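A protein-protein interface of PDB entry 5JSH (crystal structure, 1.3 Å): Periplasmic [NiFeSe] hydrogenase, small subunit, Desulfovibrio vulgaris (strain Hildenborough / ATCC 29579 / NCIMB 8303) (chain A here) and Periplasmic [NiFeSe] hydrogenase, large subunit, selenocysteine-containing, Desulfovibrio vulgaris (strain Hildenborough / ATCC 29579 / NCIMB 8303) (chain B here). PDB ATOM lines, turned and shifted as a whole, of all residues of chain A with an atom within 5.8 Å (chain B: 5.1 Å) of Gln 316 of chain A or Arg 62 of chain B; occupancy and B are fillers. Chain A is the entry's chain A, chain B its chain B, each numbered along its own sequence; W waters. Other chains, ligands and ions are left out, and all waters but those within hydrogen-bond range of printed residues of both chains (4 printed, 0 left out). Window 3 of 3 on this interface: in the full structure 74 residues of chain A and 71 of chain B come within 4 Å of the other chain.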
ATOM      1  N   TYR A 268     -14.147 -13.305   4.324  1.00  0.00           N
ATOM      2  CA  TYR A 268     -14.741 -14.635   4.183  1.00  0.00           C
ATOM      3  C   TYR A 268     -14.649 -15.176   2.751  1.00  0.00           C
ATOM      4  O   TYR A 268     -14.296 -16.343   2.539  1.00  0.00           O
ATOM      5  CB  TYR A 268     -16.188 -14.581   4.655  1.00  0.00           C
ATOM      6  CG  TYR A 268     -16.912 -15.893   4.572  1.00  0.00           C
ATOM      7  CD1 TYR A 268     -16.728 -16.874   5.537  1.00  0.00           C
ATOM      8  CD2 TYR A 268     -17.792 -16.144   3.538  1.00  0.00           C
ATOM      9  CE1 TYR A 268     -17.406 -18.061   5.478  1.00  0.00           C
ATOM     10  CE2 TYR A 268     -18.478 -17.338   3.466  1.00  0.00           C
ATOM     11  CZ  TYR A 268     -18.273 -18.295   4.438  1.00  0.00           C
ATOM     12  OH  TYR A 268     -18.960 -19.478   4.382  1.00  0.00           O
ATOM     13  N   ASP A 269     -15.005 -14.364   1.749  1.00  0.00           N
ATOM     14  CA  ASP A 269     -14.988 -14.874   0.379  1.00  0.00           C
ATOM     15  C   ASP A 269     -13.567 -15.169  -0.096  1.00  0.00           C
ATOM     16  O   ASP A 269     -13.376 -15.981  -1.011  1.00  0.00           O
ATOM     17  CB  ASP A 269     -15.636 -13.875  -0.582  1.00  0.00           C
ATOM     18  CG  ASP A 269     -17.160 -13.863  -0.508  1.00  0.00           C
ATOM     19  OD1 ASP A 269     -17.767 -14.702   0.189  1.00  0.00           O
ATOM     20  OD2 ASP A 269     -17.742 -13.004  -1.193  1.00  0.00           O
ATOM     21  N   LEU A 270     -12.573 -14.500   0.493  1.00  0.00           N
ATOM     22  CA  LEU A 270     -11.162 -14.734   0.193  1.00  0.00           C
ATOM     23  C   LEU A 270     -10.624 -15.965   0.898  1.00  0.00           C
ATOM     24  O   LEU A 270      -9.458 -16.319   0.679  1.00  0.00           O
ATOM     25  CB  LEU A 270     -10.326 -13.514   0.582  1.00  0.00           C
ATOM     26  CG  LEU A 270     -10.581 -12.227  -0.213  1.00  0.00           C
ATOM     27  CD1 LEU A 270      -9.991 -11.043   0.527  1.00  0.00           C
ATOM     28  CD2 LEU A 270      -9.988 -12.318  -1.619  1.00  0.00           C
ATOM     29  N   GLY A 271     -11.420 -16.610   1.751  1.00  0.00           N
ATOM     30  CA  GLY A 271     -11.026 -17.868   2.365  1.00  0.00           C
ATOM     31  C   GLY A 271     -10.908 -17.844   3.877  1.00  0.00           C
ATOM     32  O   GLY A 271     -10.538 -18.866   4.472  1.00  0.00           O
ATOM     33  N   CYS A 272     -11.196 -16.740   4.548  1.00  0.00           N
ATOM     34  CA  CYS A 272     -10.981 -16.667   5.985  1.00  0.00           C
ATOM     35  C   CYS A 272     -11.698 -17.795   6.732  1.00  0.00           C
ATOM     36  O   CYS A 272     -12.905 -17.989   6.585  1.00  0.00           O
ATOM     37  CB  CYS A 272     -11.467 -15.313   6.482  1.00  0.00           C
ATOM     38  SG  CYS A 272     -11.053 -15.032   8.261  1.00  0.00           S
ATOM     39  N   LYS A 273     -10.959 -18.490   7.598  1.00  0.00           N
ATOM     40  CA  LYS A 273     -11.485 -19.564   8.434  1.00  0.00           C
ATOM     41  C   LYS A 273     -11.750 -19.142   9.870  1.00  0.00           C
ATOM     42  O   LYS A 273     -11.970 -20.002  10.732  1.00  0.00           O
ATOM     43  CB  LYS A 273     -10.569 -20.789   8.393  1.00  0.00           C
ATOM     44  CG  LYS A 273     -10.281 -21.281   6.964  1.00  0.00           C
ATOM     45  CD  LYS A 273     -11.579 -21.506   6.161  1.00  0.00           C
ATOM     46  CE  LYS A 273     -11.340 -22.264   4.840  1.00  0.00           C
ATOM     47  NZ  LYS A 273     -10.303 -21.608   4.024  1.00  0.00           N
ATOM     48  N   PRO A 313      -9.521 -25.724   0.564  1.00  0.00           N
ATOM     49  CA  PRO A 313      -8.572 -24.713   0.089  1.00  0.00           C
ATOM     50  C   PRO A 313      -8.547 -23.454   0.956  1.00  0.00           C
ATOM     51  O   PRO A 313      -9.580 -23.043   1.500  1.00  0.00           O
ATOM     52  CB  PRO A 313      -9.089 -24.392  -1.312  1.00  0.00           C
ATOM     53  CG  PRO A 313      -9.818 -25.638  -1.755  1.00  0.00           C
ATOM     54  CD  PRO A 313     -10.408 -26.210  -0.507  1.00  0.00           C
ATOM     55  N   PHE A 314      -7.363 -22.847   1.076  1.00  0.00           N
ATOM     56  CA  PHE A 314      -7.190 -21.703   1.965  1.00  0.00           C
ATOM     57  C   PHE A 314      -7.823 -20.442   1.403  1.00  0.00           C
ATOM     58  O   PHE A 314      -8.195 -19.558   2.178  1.00  0.00           O
ATOM     59  CB  PHE A 314      -5.710 -21.453   2.255  1.00  0.00           C
ATOM     60  CG  PHE A 314      -5.044 -22.540   3.055  1.00  0.00           C
ATOM     61  CD1 PHE A 314      -5.577 -22.980   4.260  1.00  0.00           C
ATOM     62  CD2 PHE A 314      -3.868 -23.119   2.601  1.00  0.00           C
ATOM     63  CE1 PHE A 314      -4.956 -23.972   4.994  1.00  0.00           C
ATOM     64  CE2 PHE A 314      -3.246 -24.094   3.330  1.00  0.00           C
ATOM     65  CZ  PHE A 314      -3.786 -24.532   4.522  1.00  0.00           C
ATOM     66  N   TYR A 315      -7.931 -20.319   0.079  1.00  0.00           N
ATOM     67  CA  TYR A 315      -8.297 -19.058  -0.553  1.00  0.00           C
ATOM     68  C   TYR A 315      -9.681 -19.078  -1.193  1.00  0.00           C
ATOM     69  O   TYR A 315      -9.976 -18.263  -2.072  1.00  0.00           O
ATOM     70  CB  TYR A 315      -7.181 -18.593  -1.484  1.00  0.00           C
ATOM     71  CG  TYR A 315      -5.904 -18.346  -0.684  1.00  0.00           C
ATOM     72  CD1 TYR A 315      -5.833 -17.330   0.259  1.00  0.00           C
ATOM     73  CD2 TYR A 315      -4.797 -19.149  -0.843  1.00  0.00           C
ATOM     74  CE1 TYR A 315      -4.683 -17.109   0.989  1.00  0.00           C
ATOM     75  CE2 TYR A 315      -3.643 -18.928  -0.142  1.00  0.00           C
ATOM     76  CZ  TYR A 315      -3.591 -17.915   0.796  1.00  0.00           C
ATOM     77  OH  TYR A 315      -2.439 -17.696   1.522  1.00  0.00           O
ATOM     78  N   GLN A 316     -10.547 -19.969  -0.737  1.00  0.00           N
ATOM     79  CA  GLN A 316     -11.972 -19.815  -0.976  1.00  0.00           C
ATOM     80  C   GLN A 316     -12.720 -20.340   0.240  1.00  0.00           C
ATOM     81  O   GLN A 316     -12.153 -21.031   1.096  1.00  0.00           O
ATOM     82  CB  GLN A 316     -12.417 -20.456  -2.294  1.00  0.00           C
ATOM     83  CG  GLN A 316     -11.865 -21.810  -2.558  1.00  0.00           C
ATOM     84  CD  GLN A 316     -12.250 -22.328  -3.922  1.00  0.00           C
ATOM     85  OE1 GLN A 316     -12.053 -21.652  -4.939  1.00  0.00           O
ATOM     86  NE2 GLN A 316     -12.829 -23.519  -3.956  1.00  0.00           N
ATOM     87  N   ALA A 317     -13.989 -19.948   0.339  1.00  0.00           N
ATOM     88  CA  ALA A 317     -14.795 -20.325   1.485  1.00  0.00           C
ATOM     89  C   ALA A 317     -15.018 -21.831   1.498  1.00  0.00           C
ATOM     90  O   ALA A 317     -14.937 -22.476   2.547  1.00  0.00           O
ATOM     91  CB  ALA A 317     -16.124 -19.575   1.470  1.00  0.00           C
ATOM     92  OXT ALA A 317     -15.257 -22.437   0.453  1.00  0.00           O
ATOM     93  N   ASP B  60      -5.543 -27.357  -4.462  1.00  0.00           N
ATOM     94  CA  ASP B  60      -5.623 -26.057  -5.112  1.00  0.00           C
ATOM     95  C   ASP B  60      -4.213 -25.462  -5.150  1.00  0.00           C
ATOM     96  O   ASP B  60      -3.552 -25.389  -4.100  1.00  0.00           O
ATOM     97  CB  ASP B  60      -6.567 -25.187  -4.260  1.00  0.00           C
ATOM     98  CG  ASP B  60      -6.765 -23.762  -4.790  1.00  0.00           C
ATOM     99  OD1 ASP B  60      -5.867 -23.170  -5.427  1.00  0.00           O
ATOM    100  OD2 ASP B  60      -7.844 -23.191  -4.473  1.00  0.00           O
ATOM    101  N   PRO B  61      -3.698 -25.080  -6.325  1.00  0.00           N
ATOM    102  CA  PRO B  61      -2.293 -24.619  -6.371  1.00  0.00           C
ATOM    103  C   PRO B  61      -2.003 -23.446  -5.447  1.00  0.00           C
ATOM    104  O   PRO B  61      -0.881 -23.317  -4.939  1.00  0.00           O
ATOM    105  CB  PRO B  61      -2.092 -24.259  -7.849  1.00  0.00           C
ATOM    106  CG  PRO B  61      -3.090 -25.119  -8.568  1.00  0.00           C
ATOM    107  CD  PRO B  61      -4.303 -25.125  -7.674  1.00  0.00           C
ATOM    108  N   ARG B  62      -2.994 -22.582  -5.210  1.00  0.00           N
ATOM    109  CA  ARG B  62      -2.776 -21.430  -4.342  1.00  0.00           C
ATOM    110  C   ARG B  62      -2.440 -21.846  -2.916  1.00  0.00           C
ATOM    111  O   ARG B  62      -1.792 -21.083  -2.197  1.00  0.00           O
ATOM    112  CB  ARG B  62      -4.012 -20.534  -4.339  1.00  0.00           C
ATOM    113  CG  ARG B  62      -4.339 -19.932  -5.701  1.00  0.00           C
ATOM    114  CD  ARG B  62      -5.678 -19.247  -5.704  1.00  0.00           C
ATOM    115  NE  ARG B  62      -6.763 -20.196  -5.491  1.00  0.00           N
ATOM    116  CZ  ARG B  62      -8.046 -19.868  -5.489  1.00  0.00           C
ATOM    117  NH1 ARG B  62      -8.423 -18.617  -5.700  1.00  0.00           N
ATOM    118  NH2 ARG B  62      -8.951 -20.804  -5.281  1.00  0.00           N
ATOM    119  N   ASP B  63      -2.862 -23.034  -2.489  1.00  0.00           N
ATOM    120  CA  ASP B  63      -2.527 -23.486  -1.146  1.00  0.00           C
ATOM    121  C   ASP B  63      -1.026 -23.691  -0.976  1.00  0.00           C
ATOM    122  O   ASP B  63      -0.537 -23.689   0.161  1.00  0.00           O
ATOM    123  CB  ASP B  63      -3.195 -24.818  -0.824  1.00  0.00           C
ATOM    124  CG  ASP B  63      -4.690 -24.721  -0.631  1.00  0.00           C
ATOM    125  OD1 ASP B  63      -5.261 -23.610  -0.675  1.00  0.00           O
ATOM    126  OD2 ASP B  63      -5.300 -25.804  -0.450  1.00  0.00           O
ATOM    127  N   ALA B  64      -0.283 -23.900  -2.067  1.00  0.00           N
ATOM    128  CA  ALA B  64       1.135 -24.226  -1.947  1.00  0.00           C
ATOM    129  C   ALA B  64       1.898 -23.149  -1.193  1.00  0.00           C
ATOM    130  O   ALA B  64       2.822 -23.462  -0.438  1.00  0.00           O
ATOM    131  CB  ALA B  64       1.755 -24.447  -3.326  1.00  0.00           C
ATOM    132  N   SER B  65       1.539 -21.877  -1.394  1.00  0.00           N
ATOM    133  CA  SER B  65       2.325 -20.804  -0.807  1.00  0.00           C
ATOM    134  C   SER B  65       2.149 -20.702   0.705  1.00  0.00           C
ATOM    135  O   SER B  65       2.909 -19.970   1.341  1.00  0.00           O
ATOM    136  CB  SER B  65       2.077 -19.484  -1.535  1.00  0.00           C
ATOM    137  OG  SER B  65       0.705 -19.159  -1.605  1.00  0.00           O
ATOM    138  N   GLN B  66       1.177 -21.404   1.277  1.00  0.00           N
ATOM    139  CA  GLN B  66       1.122 -21.659   2.711  1.00  0.00           C
ATOM    140  C   GLN B  66       1.782 -22.985   3.097  1.00  0.00           C
ATOM    141  O   GLN B  66       2.619 -23.035   4.012  1.00  0.00           O
ATOM    142  CB  GLN B  66      -0.329 -21.596   3.215  1.00  0.00           C
ATOM    143  CG  GLN B  66      -0.873 -20.179   3.257  1.00  0.00           C
ATOM    144  CD  GLN B  66      -0.033 -19.298   4.136  1.00  0.00           C
ATOM    145  OE1 GLN B  66       0.164 -19.603   5.307  1.00  0.00           O
ATOM    146  NE2 GLN B  66       0.481 -18.221   3.584  1.00  0.00           N
ATOM    147  N   LEU B  87       3.971 -19.940  -8.907  1.00  0.00           N
ATOM    148  CA  LEU B  87       2.552 -19.747  -9.164  1.00  0.00           C
ATOM    149  C   LEU B  87       2.311 -18.541 -10.066  1.00  0.00           C
ATOM    150  O   LEU B  87       1.461 -18.595 -10.969  1.00  0.00           O
ATOM    151  CB  LEU B  87       1.790 -19.576  -7.849  1.00  0.00           C
ATOM    152  CG  LEU B  87       1.774 -20.781  -6.915  1.00  0.00           C
ATOM    153  CD1 LEU B  87       1.198 -20.401  -5.566  1.00  0.00           C
ATOM    154  CD2 LEU B  87       0.975 -21.927  -7.496  1.00  0.00           C
ATOM    155  N   PHE B  91       0.265 -19.141 -13.412  1.00  0.00           N
ATOM    156  CA  PHE B  91      -1.032 -18.487 -13.566  1.00  0.00           C
ATOM    157  C   PHE B  91      -1.000 -17.340 -14.572  1.00  0.00           C
ATOM    158  O   PHE B  91      -2.062 -16.822 -14.944  1.00  0.00           O
ATOM    159  CB  PHE B  91      -1.512 -17.886 -12.236  1.00  0.00           C
ATOM    160  CG  PHE B  91      -2.057 -18.869 -11.227  1.00  0.00           C
ATOM    161  CD1 PHE B  91      -1.448 -20.082 -10.966  1.00  0.00           C
ATOM    162  CD2 PHE B  91      -3.167 -18.518 -10.465  1.00  0.00           C
ATOM    163  CE1 PHE B  91      -1.948 -20.935  -9.994  1.00  0.00           C
ATOM    164  CE2 PHE B  91      -3.656 -19.364  -9.490  1.00  0.00           C
ATOM    165  CZ  PHE B  91      -3.047 -20.574  -9.257  1.00  0.00           C
ATOM    166  N   VAL B 188       0.084 -15.725  -4.825  1.00  0.00           N
ATOM    167  CA  VAL B 188       0.128 -15.535  -6.266  1.00  0.00           C
ATOM    168  C   VAL B 188      -0.458 -14.169  -6.575  1.00  0.00           C
ATOM    169  O   VAL B 188      -1.502 -13.789  -6.040  1.00  0.00           O
ATOM    170  CB  VAL B 188      -0.606 -16.678  -6.990  1.00  0.00           C
ATOM    171  CG1 VAL B 188      -2.108 -16.677  -6.697  1.00  0.00           C
ATOM    172  CG2 VAL B 188      -0.332 -16.584  -8.506  1.00  0.00           C
ATOM    173  N   VAL B 405      -7.471 -19.390 -11.326  1.00  0.00           N
ATOM    174  CA  VAL B 405      -6.655 -20.613 -11.332  1.00  0.00           C
ATOM    175  C   VAL B 405      -6.714 -21.244 -12.720  1.00  0.00           C
ATOM    176  O   VAL B 405      -7.816 -21.500 -13.228  1.00  0.00           O
ATOM    177  CB  VAL B 405      -7.165 -21.593 -10.273  1.00  0.00           C
ATOM    178  CG1 VAL B 405      -6.445 -22.931 -10.381  1.00  0.00           C
ATOM    179  CG2 VAL B 405      -7.035 -21.000  -8.874  1.00  0.00           C
HETATM  180  O   HOH W   1     -11.333 -18.472  -5.711  1.00  0.00           O
HETATM  181  O   HOH W   2       0.066 -17.667   0.630  1.00  0.00           O
HETATM  182  O   HOH W   3      -6.730 -21.841  -2.110  1.00  0.00           O
HETATM  183  O   HOH W   4     -10.284 -24.463  -4.958  1.00  0.00           O
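Of the 11 printed residues of chain A, 4 touch a printed residue of chain B. Printed residues of chain A that touch a printed residue of chain B: Pro 313, Phe 314, Tyr 315 and Gln 316. Among the printed residues, 7 pairs touch across the chains.
Water W2 lies within hydrogen-bond range of the side-chain hydroxyl of Tyr 315 of chain A (2.7 Å), the side-chain hydroxyl of Ser 65 of chain B (2.8 Å) and the side-chain amide nitrogen of Gln 66 of chain B (3.0 Å). Water W3 lies within hydrogen-bond range of OD1 of Asp 63 of chain B (2.7 Å), N of Tyr 315 of chain A (2.9 Å), OD2 of Asp 60 of chain B (2.9 Å) and N of Phe 314 of chain A (3.4 Å). Water W4 bridges OD2 of Asp 60 of chain B (2.8 Å) and NE2 of Gln 316 of chain A (2.9 Å). Water W1 bridges the guanidinium group (NH1) of Arg 62 of chain B and the side-chain amide oxygen (OE1) of Gln 316 of chain A.
The side-chain amino group (NZ) of Lys 273 of chain A sits at hydrogen-bond distance from the backbone carbonyl oxygen (O) of Pro 313 of chain A, at 3.0 Å. O of Phe 314 of chain A is in hydrogen-bond range of NZ of Lys 273 of chain A. NH2 of Arg 62 of chain B lies within salt-bridge range of OD2 of Asp 60 of chain B, at 2.8 Å. The backbone carbonyl oxygen (O) of Arg 62 of chain B is in hydrogen-bond range of the side-chain hydroxyl (OG) of Ser 65 of chain B (3.2 Å).
OD2 of Asp 60 of chain B touches CB of Pro 313 of chain A (3.6 Å). Pro 313 of chain A touches Asp 63 of chain B (CA to OD2, 3.5 Å). CE2 of Phe 314 of chain A touches CB of Gln 66 of chain B, 3.8 Å away. Tyr 315 of chain A touches Arg 62 of chain B. Gln 66 of chain B touches Tyr 315 of chain A (CG to OH, 3.4 Å).
The backbone NH (N) of Phe 314 of chain A is in hydrogen-bond range of the side-chain carboxylate (OD1) of Asp 63 of chain B (2.8 Å). OE1 of Gln 316 of chain A lies within hydrogen-bond range of NH2 of Arg 62 of chain B, at 3.2 Å.
Of the printed residues of chain B, Pro 313 of chain A touches Asp 60 (3.6 Å) and Asp 63 (3.5 Å). Of the printed residues of chain B, Tyr 315 of chain A touches Arg 62 and Gln 66. Gln 316 of chain A touches just one residue of chain B: Arg 62 (3.2 Å). Arg 62 of chain B touches just these residues of chain A: Tyr 315 (3.5 Å) and Gln 316 (3.2 Å). The nearest residue of chain B that does not touch Gln 316 of chain A is Asp 60 of chain B (4.5 Å).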
